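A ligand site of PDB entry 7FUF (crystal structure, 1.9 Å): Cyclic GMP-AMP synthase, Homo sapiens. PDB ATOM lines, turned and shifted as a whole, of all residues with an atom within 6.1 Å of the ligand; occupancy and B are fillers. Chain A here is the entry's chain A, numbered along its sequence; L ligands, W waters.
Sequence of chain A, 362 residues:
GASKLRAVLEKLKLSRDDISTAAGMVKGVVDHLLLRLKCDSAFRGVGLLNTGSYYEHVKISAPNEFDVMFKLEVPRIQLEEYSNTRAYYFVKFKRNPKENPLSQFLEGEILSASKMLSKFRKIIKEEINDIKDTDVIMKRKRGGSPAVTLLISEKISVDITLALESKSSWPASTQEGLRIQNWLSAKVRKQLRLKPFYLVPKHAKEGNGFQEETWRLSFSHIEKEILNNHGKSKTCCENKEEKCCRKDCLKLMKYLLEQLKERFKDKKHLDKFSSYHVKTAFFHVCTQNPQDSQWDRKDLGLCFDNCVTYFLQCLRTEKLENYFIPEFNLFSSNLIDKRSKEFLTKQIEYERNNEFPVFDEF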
ATOM      1  N   THR A  85      20.660  18.650  12.501  1.00  0.00           N
ATOM      2  CA  THR A  85      20.826  18.489  13.948  1.00  0.00           C
ATOM      3  C   THR A  85      21.371  17.126  14.338  1.00  0.00           C
ATOM      4  O   THR A  85      21.724  16.941  15.501  1.00  0.00           O
ATOM      5  CB  THR A  85      19.496  18.728  14.663  1.00  0.00           C
ATOM      6  OG1 THR A  85      18.505  17.845  14.137  1.00  0.00           O
ATOM      7  CG2 THR A  85      19.044  20.163  14.455  1.00  0.00           C
ATOM      8  N   ARG A  86      21.431  16.184  13.395  1.00  0.00           N
ATOM      9  CA  ARG A  86      21.920  14.814  13.605  1.00  0.00           C
ATOM     10  C   ARG A  86      21.004  13.961  14.487  1.00  0.00           C
ATOM     11  O   ARG A  86      21.007  12.718  14.361  1.00  0.00           O
ATOM     12  CB  ARG A  86      23.350  14.823  14.177  1.00  0.00           C
ATOM     13  CG  ARG A  86      24.385  15.608  13.342  1.00  0.00           C
ATOM     14  CD  ARG A  86      25.117  14.763  12.286  1.00  0.00           C
ATOM     15  NE  ARG A  86      24.206  14.210  11.277  1.00  0.00           N
ATOM     16  CZ  ARG A  86      24.534  13.258  10.406  1.00  0.00           C
ATOM     17  NH1 ARG A  86      25.761  12.753  10.410  1.00  0.00           N
ATOM     18  NH2 ARG A  86      23.635  12.812   9.532  1.00  0.00           N
ATOM     19  N   ALA A  87      20.208  14.583  15.356  1.00  0.00           N
ATOM     20  CA  ALA A  87      19.380  13.850  16.306  1.00  0.00           C
ATOM     21  C   ALA A  87      17.882  14.024  16.105  1.00  0.00           C
ATOM     22  O   ALA A  87      17.104  13.224  16.650  1.00  0.00           O
ATOM     23  CB  ALA A  87      19.738  14.278  17.738  1.00  0.00           C
ATOM     24  N   TYR A  88      17.438  15.028  15.360  1.00  0.00           N
ATOM     25  CA  TYR A  88      16.033  15.348  15.211  1.00  0.00           C
ATOM     26  C   TYR A  88      15.591  15.089  13.776  1.00  0.00           C
ATOM     27  O   TYR A  88      16.311  15.454  12.830  1.00  0.00           O
ATOM     28  CB  TYR A  88      15.767  16.797  15.622  1.00  0.00           C
ATOM     29  CG  TYR A  88      16.114  17.073  17.086  1.00  0.00           C
ATOM     30  CD1 TYR A  88      17.302  17.673  17.455  1.00  0.00           C
ATOM     31  CD2 TYR A  88      15.215  16.698  18.103  1.00  0.00           C
ATOM     32  CE1 TYR A  88      17.616  17.906  18.789  1.00  0.00           C
ATOM     33  CE2 TYR A  88      15.506  16.931  19.440  1.00  0.00           C
ATOM     34  CZ  TYR A  88      16.713  17.527  19.772  1.00  0.00           C
ATOM     35  OH  TYR A  88      17.022  17.765  21.094  1.00  0.00           O
ATOM     36  N   LEU A 178      28.610   4.277  19.348  1.00  0.00           N
ATOM     37  CA  LEU A 178      28.666   3.005  20.052  1.00  0.00           C
ATOM     38  C   LEU A 178      30.071   2.395  19.945  1.00  0.00           C
ATOM     39  O   LEU A 178      30.266   1.256  19.520  1.00  0.00           O
ATOM     40  CB  LEU A 178      27.577   2.062  19.532  1.00  0.00           C
ATOM     41  CG  LEU A 178      27.199   0.865  20.397  1.00  0.00           C
ATOM     42  CD1 LEU A 178      26.693   1.355  21.751  1.00  0.00           C
ATOM     43  CD2 LEU A 178      26.164   0.141  19.699  1.00  0.00           C
ATOM     44  N   ARG A 216      13.049  12.769  18.113  1.00  0.00           N
ATOM     45  CA  ARG A 216      14.432  12.568  18.530  1.00  0.00           C
ATOM     46  C   ARG A 216      14.745  11.075  18.580  1.00  0.00           C
ATOM     47  O   ARG A 216      13.897  10.281  18.993  1.00  0.00           O
ATOM     48  CB  ARG A 216      14.672  13.213  19.906  1.00  0.00           C
ATOM     49  CG  ARG A 216      16.003  12.924  20.516  1.00  0.00           C
ATOM     50  CD  ARG A 216      16.199  13.612  21.856  1.00  0.00           C
ATOM     51  NE  ARG A 216      15.272  13.183  22.898  1.00  0.00           N
ATOM     52  CZ  ARG A 216      15.276  11.992  23.485  1.00  0.00           C
ATOM     53  NH1 ARG A 216      16.160  11.044  23.144  1.00  0.00           N
ATOM     54  NH2 ARG A 216      14.405  11.745  24.442  1.00  0.00           N
ATOM     55  N   LEU A 217      15.941  10.681  18.146  1.00  0.00           N
ATOM     56  CA  LEU A 217      16.356   9.291  18.282  1.00  0.00           C
ATOM     57  C   LEU A 217      16.522   8.924  19.750  1.00  0.00           C
ATOM     58  O   LEU A 217      17.043   9.719  20.545  1.00  0.00           O
ATOM     59  CB  LEU A 217      17.683   9.063  17.548  1.00  0.00           C
ATOM     60  CG  LEU A 217      17.633   9.238  16.022  1.00  0.00           C
ATOM     61  CD1 LEU A 217      18.999   9.030  15.361  1.00  0.00           C
ATOM     62  CD2 LEU A 217      16.609   8.271  15.466  1.00  0.00           C
ATOM     63  N   SER A 218      16.098   7.705  20.100  1.00  0.00           N
ATOM     64  CA  SER A 218      16.117   7.190  21.465  1.00  0.00           C
ATOM     65  C   SER A 218      16.752   5.811  21.495  1.00  0.00           C
ATOM     66  O   SER A 218      16.357   4.936  20.711  1.00  0.00           O
ATOM     67  CB  SER A 218      14.712   7.077  22.046  1.00  0.00           C
ATOM     68  OG  SER A 218      14.743   6.683  23.409  1.00  0.00           O
ATOM     69  N   PHE A 219      17.679   5.592  22.410  1.00  0.00           N
ATOM     70  CA  PHE A 219      18.296   4.280  22.598  1.00  0.00           C
ATOM     71  C   PHE A 219      18.209   3.839  24.051  1.00  0.00           C
ATOM     72  O   PHE A 219      19.184   3.366  24.650  1.00  0.00           O
ATOM     73  CB  PHE A 219      19.752   4.326  22.133  1.00  0.00           C
ATOM     74  CG  PHE A 219      19.890   4.694  20.707  1.00  0.00           C
ATOM     75  CD1 PHE A 219      19.738   3.739  19.721  1.00  0.00           C
ATOM     76  CD2 PHE A 219      20.149   5.998  20.334  1.00  0.00           C
ATOM     77  CE1 PHE A 219      19.853   4.070  18.393  1.00  0.00           C
ATOM     78  CE2 PHE A 219      20.255   6.343  18.999  1.00  0.00           C
ATOM     79  CZ  PHE A 219      20.115   5.377  18.037  1.00  0.00           C
ATOM     80  N   SER A 220      17.009   3.963  24.640  1.00  0.00           N
ATOM     81  CA  SER A 220      16.801   3.715  26.070  1.00  0.00           C
ATOM     82  C   SER A 220      16.895   2.247  26.421  1.00  0.00           C
ATOM     83  O   SER A 220      16.819   1.902  27.603  1.00  0.00           O
ATOM     84  CB  SER A 220      15.437   4.260  26.494  1.00  0.00           C
ATOM     85  OG  SER A 220      14.403   3.594  25.804  1.00  0.00           O
ATOM     86  N   HIS A 221      17.044   1.381  25.440  1.00  0.00           N
ATOM     87  CA  HIS A 221      17.097  -0.047  25.685  1.00  0.00           C
ATOM     88  C   HIS A 221      18.495  -0.604  25.647  1.00  0.00           C
ATOM     89  O   HIS A 221      18.678  -1.785  25.892  1.00  0.00           O
ATOM     90  CB  HIS A 221      16.250  -0.788  24.653  1.00  0.00           C
ATOM     91  CG  HIS A 221      16.687  -0.538  23.235  1.00  0.00           C
ATOM     92  ND1 HIS A 221      17.055   0.708  22.790  1.00  0.00           N
ATOM     93  CD2 HIS A 221      16.795  -1.369  22.173  1.00  0.00           C
ATOM     94  CE1 HIS A 221      17.362   0.636  21.501  1.00  0.00           C
ATOM     95  NE2 HIS A 221      17.219  -0.616  21.104  1.00  0.00           N
ATOM     96  N   ILE A 222      19.497   0.219  25.348  1.00  0.00           N
ATOM     97  CA  ILE A 222      20.845  -0.281  25.173  1.00  0.00           C
ATOM     98  C   ILE A 222      21.567  -0.408  26.507  1.00  0.00           C
ATOM     99  O   ILE A 222      22.328  -1.352  26.734  1.00  0.00           O
ATOM    100  CB  ILE A 222      21.605   0.651  24.226  1.00  0.00           C
ATOM    101  CG1 ILE A 222      20.917   0.667  22.869  1.00  0.00           C
ATOM    102  CG2 ILE A 222      23.046   0.221  24.121  1.00  0.00           C
ATOM    103  CD1 ILE A 222      20.856  -0.672  22.213  1.00  0.00           C
ATOM    104  N   GLU A 223      21.359   0.552  27.405  1.00  0.00           N
ATOM    105  CA  GLU A 223      22.051   0.566  28.681  1.00  0.00           C
ATOM    106  C   GLU A 223      21.896  -0.752  29.412  1.00  0.00           C
ATOM    107  O   GLU A 223      22.859  -1.283  29.957  1.00  0.00           O
ATOM    108  CB  GLU A 223      21.508   1.699  29.561  1.00  0.00           C
ATOM    109  CG  GLU A 223      22.124   1.650  30.958  1.00  0.00           C
ATOM    110  CD  GLU A 223      21.544   2.661  31.941  1.00  0.00           C
ATOM    111  OE1 GLU A 223      22.287   3.086  32.843  1.00  0.00           O
ATOM    112  OE2 GLU A 223      20.351   3.023  31.830  1.00  0.00           O
ATOM    113  N   ILE A 226      24.116  -3.519  27.839  1.00  0.00           N
ATOM    114  CA  ILE A 226      25.511  -3.405  28.212  1.00  0.00           C
ATOM    115  C   ILE A 226      25.710  -3.756  29.678  1.00  0.00           C
ATOM    116  O   ILE A 226      26.625  -4.512  30.029  1.00  0.00           O
ATOM    117  CB  ILE A 226      26.000  -1.989  27.916  1.00  0.00           C
ATOM    118  CG1 ILE A 226      25.992  -1.802  26.417  1.00  0.00           C
ATOM    119  CG2 ILE A 226      27.351  -1.741  28.576  1.00  0.00           C
ATOM    120  CD1 ILE A 226      26.213  -0.380  26.072  1.00  0.00           C
ATOM    121  N   SER A 274      21.021  15.949  33.704  1.00  0.00           N
ATOM    122  CA  SER A 274      20.240  14.794  34.127  1.00  0.00           C
ATOM    123  C   SER A 274      21.073  13.531  33.979  1.00  0.00           C
ATOM    124  O   SER A 274      22.211  13.558  33.506  1.00  0.00           O
ATOM    125  CB  SER A 274      18.934  14.713  33.340  1.00  0.00           C
ATOM    126  OG  SER A 274      19.214  14.383  32.002  1.00  0.00           O
ATOM    127  N   TYR A 276      21.204  11.013  32.071  1.00  0.00           N
ATOM    128  CA  TYR A 276      21.819  10.513  30.862  1.00  0.00           C
ATOM    129  C   TYR A 276      23.110  11.248  30.538  1.00  0.00           C
ATOM    130  O   TYR A 276      23.958  10.697  29.845  1.00  0.00           O
ATOM    131  CB  TYR A 276      20.831  10.536  29.703  1.00  0.00           C
ATOM    132  CG  TYR A 276      20.665  11.853  29.032  1.00  0.00           C
ATOM    133  CD1 TYR A 276      19.734  12.775  29.497  1.00  0.00           C
ATOM    134  CD2 TYR A 276      21.410  12.184  27.904  1.00  0.00           C
ATOM    135  CE1 TYR A 276      19.557  14.011  28.864  1.00  0.00           C
ATOM    136  CE2 TYR A 276      21.245  13.428  27.268  1.00  0.00           C
ATOM    137  CZ  TYR A 276      20.320  14.331  27.746  1.00  0.00           C
ATOM    138  OH  TYR A 276      20.144  15.553  27.115  1.00  0.00           O
ATOM    139  N   LYS A 279      25.356   8.989  32.599  1.00  0.00           N
ATOM    140  CA  LYS A 279      25.475   7.735  31.855  1.00  0.00           C
ATOM    141  C   LYS A 279      26.441   7.870  30.706  1.00  0.00           C
ATOM    142  O   LYS A 279      27.365   7.059  30.550  1.00  0.00           O
ATOM    143  CB  LYS A 279      24.100   7.295  31.354  1.00  0.00           C
ATOM    144  CG  LYS A 279      23.152   6.823  32.446  1.00  0.00           C
ATOM    145  CD  LYS A 279      21.804   6.424  31.881  1.00  0.00           C
ATOM    146  CE  LYS A 279      20.826   6.196  33.029  1.00  0.00           C
ATOM    147  NZ  LYS A 279      19.555   5.622  32.526  1.00  0.00           N
ATOM    148  N   THR A 280      26.246   8.895  29.861  1.00  0.00           N
ATOM    149  CA  THR A 280      27.113   9.113  28.714  1.00  0.00           C
ATOM    150  C   THR A 280      28.575   9.183  29.118  1.00  0.00           C
ATOM    151  O   THR A 280      29.430   8.501  28.550  1.00  0.00           O
ATOM    152  CB  THR A 280      26.701  10.388  28.004  1.00  0.00           C
ATOM    153  OG1 THR A 280      25.360  10.249  27.550  1.00  0.00           O
ATOM    154  CG2 THR A 280      27.622  10.632  26.833  1.00  0.00           C
ATOM    155  N   PHE A 283      30.045   5.772  30.295  1.00  0.00           N
ATOM    156  CA  PHE A 283      30.372   4.777  29.278  1.00  0.00           C
ATOM    157  C   PHE A 283      31.503   5.234  28.384  1.00  0.00           C
ATOM    158  O   PHE A 283      32.201   4.388  27.807  1.00  0.00           O
ATOM    159  CB  PHE A 283      29.125   4.399  28.457  1.00  0.00           C
ATOM    160  CG  PHE A 283      28.127   3.556  29.232  1.00  0.00           C
ATOM    161  CD1 PHE A 283      28.421   2.243  29.575  1.00  0.00           C
ATOM    162  CD2 PHE A 283      26.879   4.068  29.608  1.00  0.00           C
ATOM    163  CE1 PHE A 283      27.512   1.465  30.290  1.00  0.00           C
ATOM    164  CE2 PHE A 283      25.959   3.283  30.326  1.00  0.00           C
ATOM    165  CZ  PHE A 283      26.294   1.986  30.672  1.00  0.00           C
ATOM    166  N   ASN A 322      27.451  12.695  22.536  1.00  0.00           N
ATOM    167  CA  ASN A 322      26.436  11.652  22.658  1.00  0.00           C
ATOM    168  C   ASN A 322      27.080  10.322  22.295  1.00  0.00           C
ATOM    169  O   ASN A 322      27.934  10.251  21.420  1.00  0.00           O
ATOM    170  CB  ASN A 322      25.256  11.942  21.741  1.00  0.00           C
ATOM    171  CG  ASN A 322      24.154  10.913  21.881  1.00  0.00           C
ATOM    172  OD1 ASN A 322      24.172   9.877  21.224  1.00  0.00           O
ATOM    173  ND2 ASN A 322      23.183  11.197  22.723  1.00  0.00           N
ATOM    174  N   TYR A 323      26.679   9.274  23.017  1.00  0.00           N
ATOM    175  CA  TYR A 323      27.367   7.996  22.893  1.00  0.00           C
ATOM    176  C   TYR A 323      27.040   7.319  21.565  1.00  0.00           C
ATOM    177  O   TYR A 323      27.844   6.523  21.058  1.00  0.00           O
ATOM    178  CB  TYR A 323      27.015   7.084  24.076  1.00  0.00           C
ATOM    179  CG  TYR A 323      28.054   6.010  24.333  1.00  0.00           C
ATOM    180  CD1 TYR A 323      29.284   6.331  24.881  1.00  0.00           C
ATOM    181  CD2 TYR A 323      27.804   4.676  23.988  1.00  0.00           C
ATOM    182  CE1 TYR A 323      30.247   5.372  25.109  1.00  0.00           C
ATOM    183  CE2 TYR A 323      28.762   3.708  24.206  1.00  0.00           C
ATOM    184  CZ  TYR A 323      29.970   4.060  24.771  1.00  0.00           C
ATOM    185  OH  TYR A 323      30.900   3.100  24.998  1.00  0.00           O
ATOM    186  N   PHE A 324      25.873   7.635  21.002  1.00  0.00           N
ATOM    187  CA  PHE A 324      25.352   7.033  19.781  1.00  0.00           C
ATOM    188  C   PHE A 324      25.558   7.906  18.561  1.00  0.00           C
ATOM    189  O   PHE A 324      25.756   7.387  17.454  1.00  0.00           O
ATOM    190  CB  PHE A 324      23.864   6.745  19.976  1.00  0.00           C
ATOM    191  CG  PHE A 324      23.604   5.800  21.114  1.00  0.00           C
ATOM    192  CD1 PHE A 324      23.591   4.438  20.910  1.00  0.00           C
ATOM    193  CD2 PHE A 324      23.459   6.276  22.398  1.00  0.00           C
ATOM    194  CE1 PHE A 324      23.421   3.562  21.965  1.00  0.00           C
ATOM    195  CE2 PHE A 324      23.297   5.415  23.455  1.00  0.00           C
ATOM    196  CZ  PHE A 324      23.278   4.058  23.238  1.00  0.00           C
ATOM    197  N   ILE A 325      25.540   9.215  18.749  1.00  0.00           N
ATOM    198  CA  ILE A 325      25.621  10.182  17.653  1.00  0.00           C
ATOM    199  C   ILE A 325      26.777  11.089  18.020  1.00  0.00           C
ATOM    200  O   ILE A 325      26.566  12.131  18.658  1.00  0.00           O
ATOM    201  CB  ILE A 325      24.289  10.925  17.491  1.00  0.00           C
ATOM    202  CG1 ILE A 325      23.151   9.936  17.240  1.00  0.00           C
ATOM    203  CG2 ILE A 325      24.363  11.994  16.409  1.00  0.00           C
ATOM    204  CD1 ILE A 325      21.799  10.585  17.073  1.00  0.00           C
ATOM    205  N   PHE A 328      26.959  14.997  18.133  1.00  0.00           N
ATOM    206  CA  PHE A 328      26.038  15.796  18.922  1.00  0.00           C
ATOM    207  C   PHE A 328      26.679  16.073  20.288  1.00  0.00           C
ATOM    208  O   PHE A 328      26.924  15.145  21.058  1.00  0.00           O
ATOM    209  CB  PHE A 328      24.691  15.099  19.077  1.00  0.00           C
ATOM    210  CG  PHE A 328      23.591  16.005  19.570  1.00  0.00           C
ATOM    211  CD1 PHE A 328      23.518  16.388  20.886  1.00  0.00           C
ATOM    212  CD2 PHE A 328      22.625  16.467  18.706  1.00  0.00           C
ATOM    213  CE1 PHE A 328      22.505  17.239  21.327  1.00  0.00           C
ATOM    214  CE2 PHE A 328      21.610  17.302  19.132  1.00  0.00           C
ATOM    215  CZ  PHE A 328      21.555  17.687  20.457  1.00  0.00           C
ATOM    216  N   LEU A 330      26.402  17.196  23.837  1.00  0.00           N
ATOM    217  CA  LEU A 330      25.445  17.436  24.908  1.00  0.00           C
ATOM    218  C   LEU A 330      25.770  18.673  25.735  1.00  0.00           C
ATOM    219  O   LEU A 330      24.869  19.222  26.378  1.00  0.00           O
ATOM    220  CB  LEU A 330      25.374  16.215  25.837  1.00  0.00           C
ATOM    221  CG  LEU A 330      24.999  14.919  25.103  1.00  0.00           C
ATOM    222  CD1 LEU A 330      25.029  13.718  26.049  1.00  0.00           C
ATOM    223  CD2 LEU A 330      23.653  15.074  24.416  1.00  0.00           C
HETATM  224  C1  LIG L   1      21.647   7.512  26.582  1.00  0.00           C
HETATM  225  C2  LIG L   1      19.371  12.012  22.740  1.00  0.00           C
HETATM  226  C3  LIG L   1      19.228  13.267  23.351  1.00  0.00           C
HETATM  227  C4  LIG L   1      19.944  14.343  22.850  1.00  0.00           C
HETATM  228  C5  LIG L   1      20.811  14.173  21.787  1.00  0.00           C
HETATM  229  C6  LIG L   1      20.946  12.931  21.210  1.00  0.00           C
HETATM  230  C7  LIG L   1      18.386  13.422  24.549  1.00  0.00           C
HETATM  231  C8  LIG L   1      17.737  14.584  25.028  1.00  0.00           C
HETATM  232  C9  LIG L   1      17.078  14.190  26.153  1.00  0.00           C
HETATM  233  C10 LIG L   1      16.871  11.995  27.384  1.00  0.00           C
HETATM  234  C11 LIG L   1      23.544   6.172  27.359  1.00  0.00           C
HETATM  235  C12 LIG L   1      24.880   6.306  27.028  1.00  0.00           C
HETATM  236  C13 LIG L   1      20.238  11.818  21.657  1.00  0.00           C
HETATM  237  C14 LIG L   1      21.075   8.390  24.464  1.00  0.00           C
HETATM  238  C15 LIG L   1      22.700   7.385  27.653  1.00  0.00           C
HETATM  239  C16 LIG L   1      20.424  10.472  21.000  1.00  0.00           C
HETATM  240  C17 LIG L   1      25.657   5.191  26.735  1.00  0.00           C
HETATM  241  C18 LIG L   1      25.101   3.930  26.792  1.00  0.00           C
HETATM  242  C19 LIG L   1      23.769   3.788  27.118  1.00  0.00           C
HETATM  243  C20 LIG L   1      22.989   4.901  27.394  1.00  0.00           C
HETATM  244  C21 LIG L   1      19.973   8.836  22.766  1.00  0.00           C
HETATM  245  C22 LIG L   1      19.413   7.107  25.680  1.00  0.00           C
HETATM  246  C23 LIG L   1      20.405   6.962  26.698  1.00  0.00           C
HETATM  247  N1  LIG L   1      21.981   8.225  25.456  1.00  0.00           N
HETATM  248  N2  LIG L   1      21.213   9.044  23.318  1.00  0.00           N
HETATM  249  N3  LIG L   1      17.340  12.870  26.313  1.00  0.00           N
HETATM  250  N4  LIG L   1      18.149  12.369  25.346  1.00  0.00           N
HETATM  251  N5  LIG L   1      19.660   9.360  21.562  1.00  0.00           N
HETATM  252  N6  LIG L   1      19.107   8.122  23.470  1.00  0.00           N
HETATM  253  N7  LIG L   1      19.858   7.840  24.576  1.00  0.00           N
HETATM  254  O1  LIG L   1      18.257   6.661  25.713  1.00  0.00           O
HETATM  255 CL1  LIG L   1      22.036  12.755  19.877  1.00  0.00          CL
HETATM  256  O   HOH W   1      17.267   6.552  28.404  1.00  0.00           O
HETATM  257  O   HOH W   2      24.621   9.328  25.112  1.00  0.00           O
HETATM  258  O   HOH W   3      15.974   8.129  25.146  1.00  0.00           O
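O of Leu 217 sits at hydrogen-bond distance from N5 of the ligand (2.8 Å). The side-chain amide nitrogen (ND2) of Asn 322 lies within hydrogen-bond range of a nitrogen (N2) of the ligand, 3.0 Å away. N of Phe 219 sits at hydrogen-bond distance from N6 of the ligand (3.1 Å). The backbone NH (N) of Ser 220 sits at hydrogen-bond distance from an oxygen (O1) of the ligand, 3.2 Å away. NH1 of Arg 216 lies within hydrogen-bond range of N4 of the ligand (3.2 Å).
The backbone NH of Leu 217 lies within hydrogen-bond range of the backbone carbonyl oxygen of Ala 87 (3.2 Å). The backbone NH of Asn 322 lies within hydrogen-bond range of the backbone carbonyl oxygen of Phe 328, at 2.9 Å. OD1 of Asn 322 is in hydrogen-bond range of N of Ile 325, 2.9 Å away. OD1 of Asn 322 lies within hydrogen-bond range of N of Phe 324 (2.8 Å). The backbone carbonyl oxygen (O) of Phe 283 is in hydrogen-bond range of the side-chain hydroxyl (OH) of Tyr 323, at 3.4 Å. O of Tyr 276 sits at hydrogen-bond distance from OG1 of Thr 280, 2.7 Å away. O of Tyr 323 lies within hydrogen-bond range of N of Leu 178. OE2 of Glu 223 lies within salt-bridge range of NZ of Lys 279 (2.8 Å).
Ala 87 touches the ligand. CA of Ser 218 touches N6 of the ligand, 3.7 Å away. Glu 223 touches the ligand. Tyr 276 touches the ligand (OH to C8, 3.3 Å). Lys 279 touches the ligand. Thr 280 touches the ligand. Phe 283 touches the ligand (CD2 to C17, 3.3 Å). Tyr 323 touches the ligand (CG to C17, 3.5 Å). Phe 324 touches the ligand (CD2 to N2, 3.7 Å). Ile 325 touches the ligand. Phe 328 touches the ligand (CE1 to C5, 3.5 Å). Leu 330 touches the ligand (CD2 to C5, 3.97 Å). Hydrophobic or aromatic side chains within 4 Å of the ligand: Ala 87, Phe 219, Tyr 276, Phe 283, Tyr 323, Phe 324, Ile 325, Phe 328 and Leu 330. 17 residues have an atom within 4 Å of the ligand: Ala 87, Arg 216, Leu 217, Ser 218, Phe 219, Ser 220, Glu 223, Tyr 276, Lys 279, Thr 280, Phe 283, Asn 322, Tyr 323, Phe 324, Ile 325, Phe 328 and Leu 330. Along chain A the residues within 4 Å of the ligand span positions 87 to 330.
Water W3 bridges the side-chain hydroxyl of Ser 218 (2.6 Å) and an oxygen (O1) of the ligand (2.8 Å).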
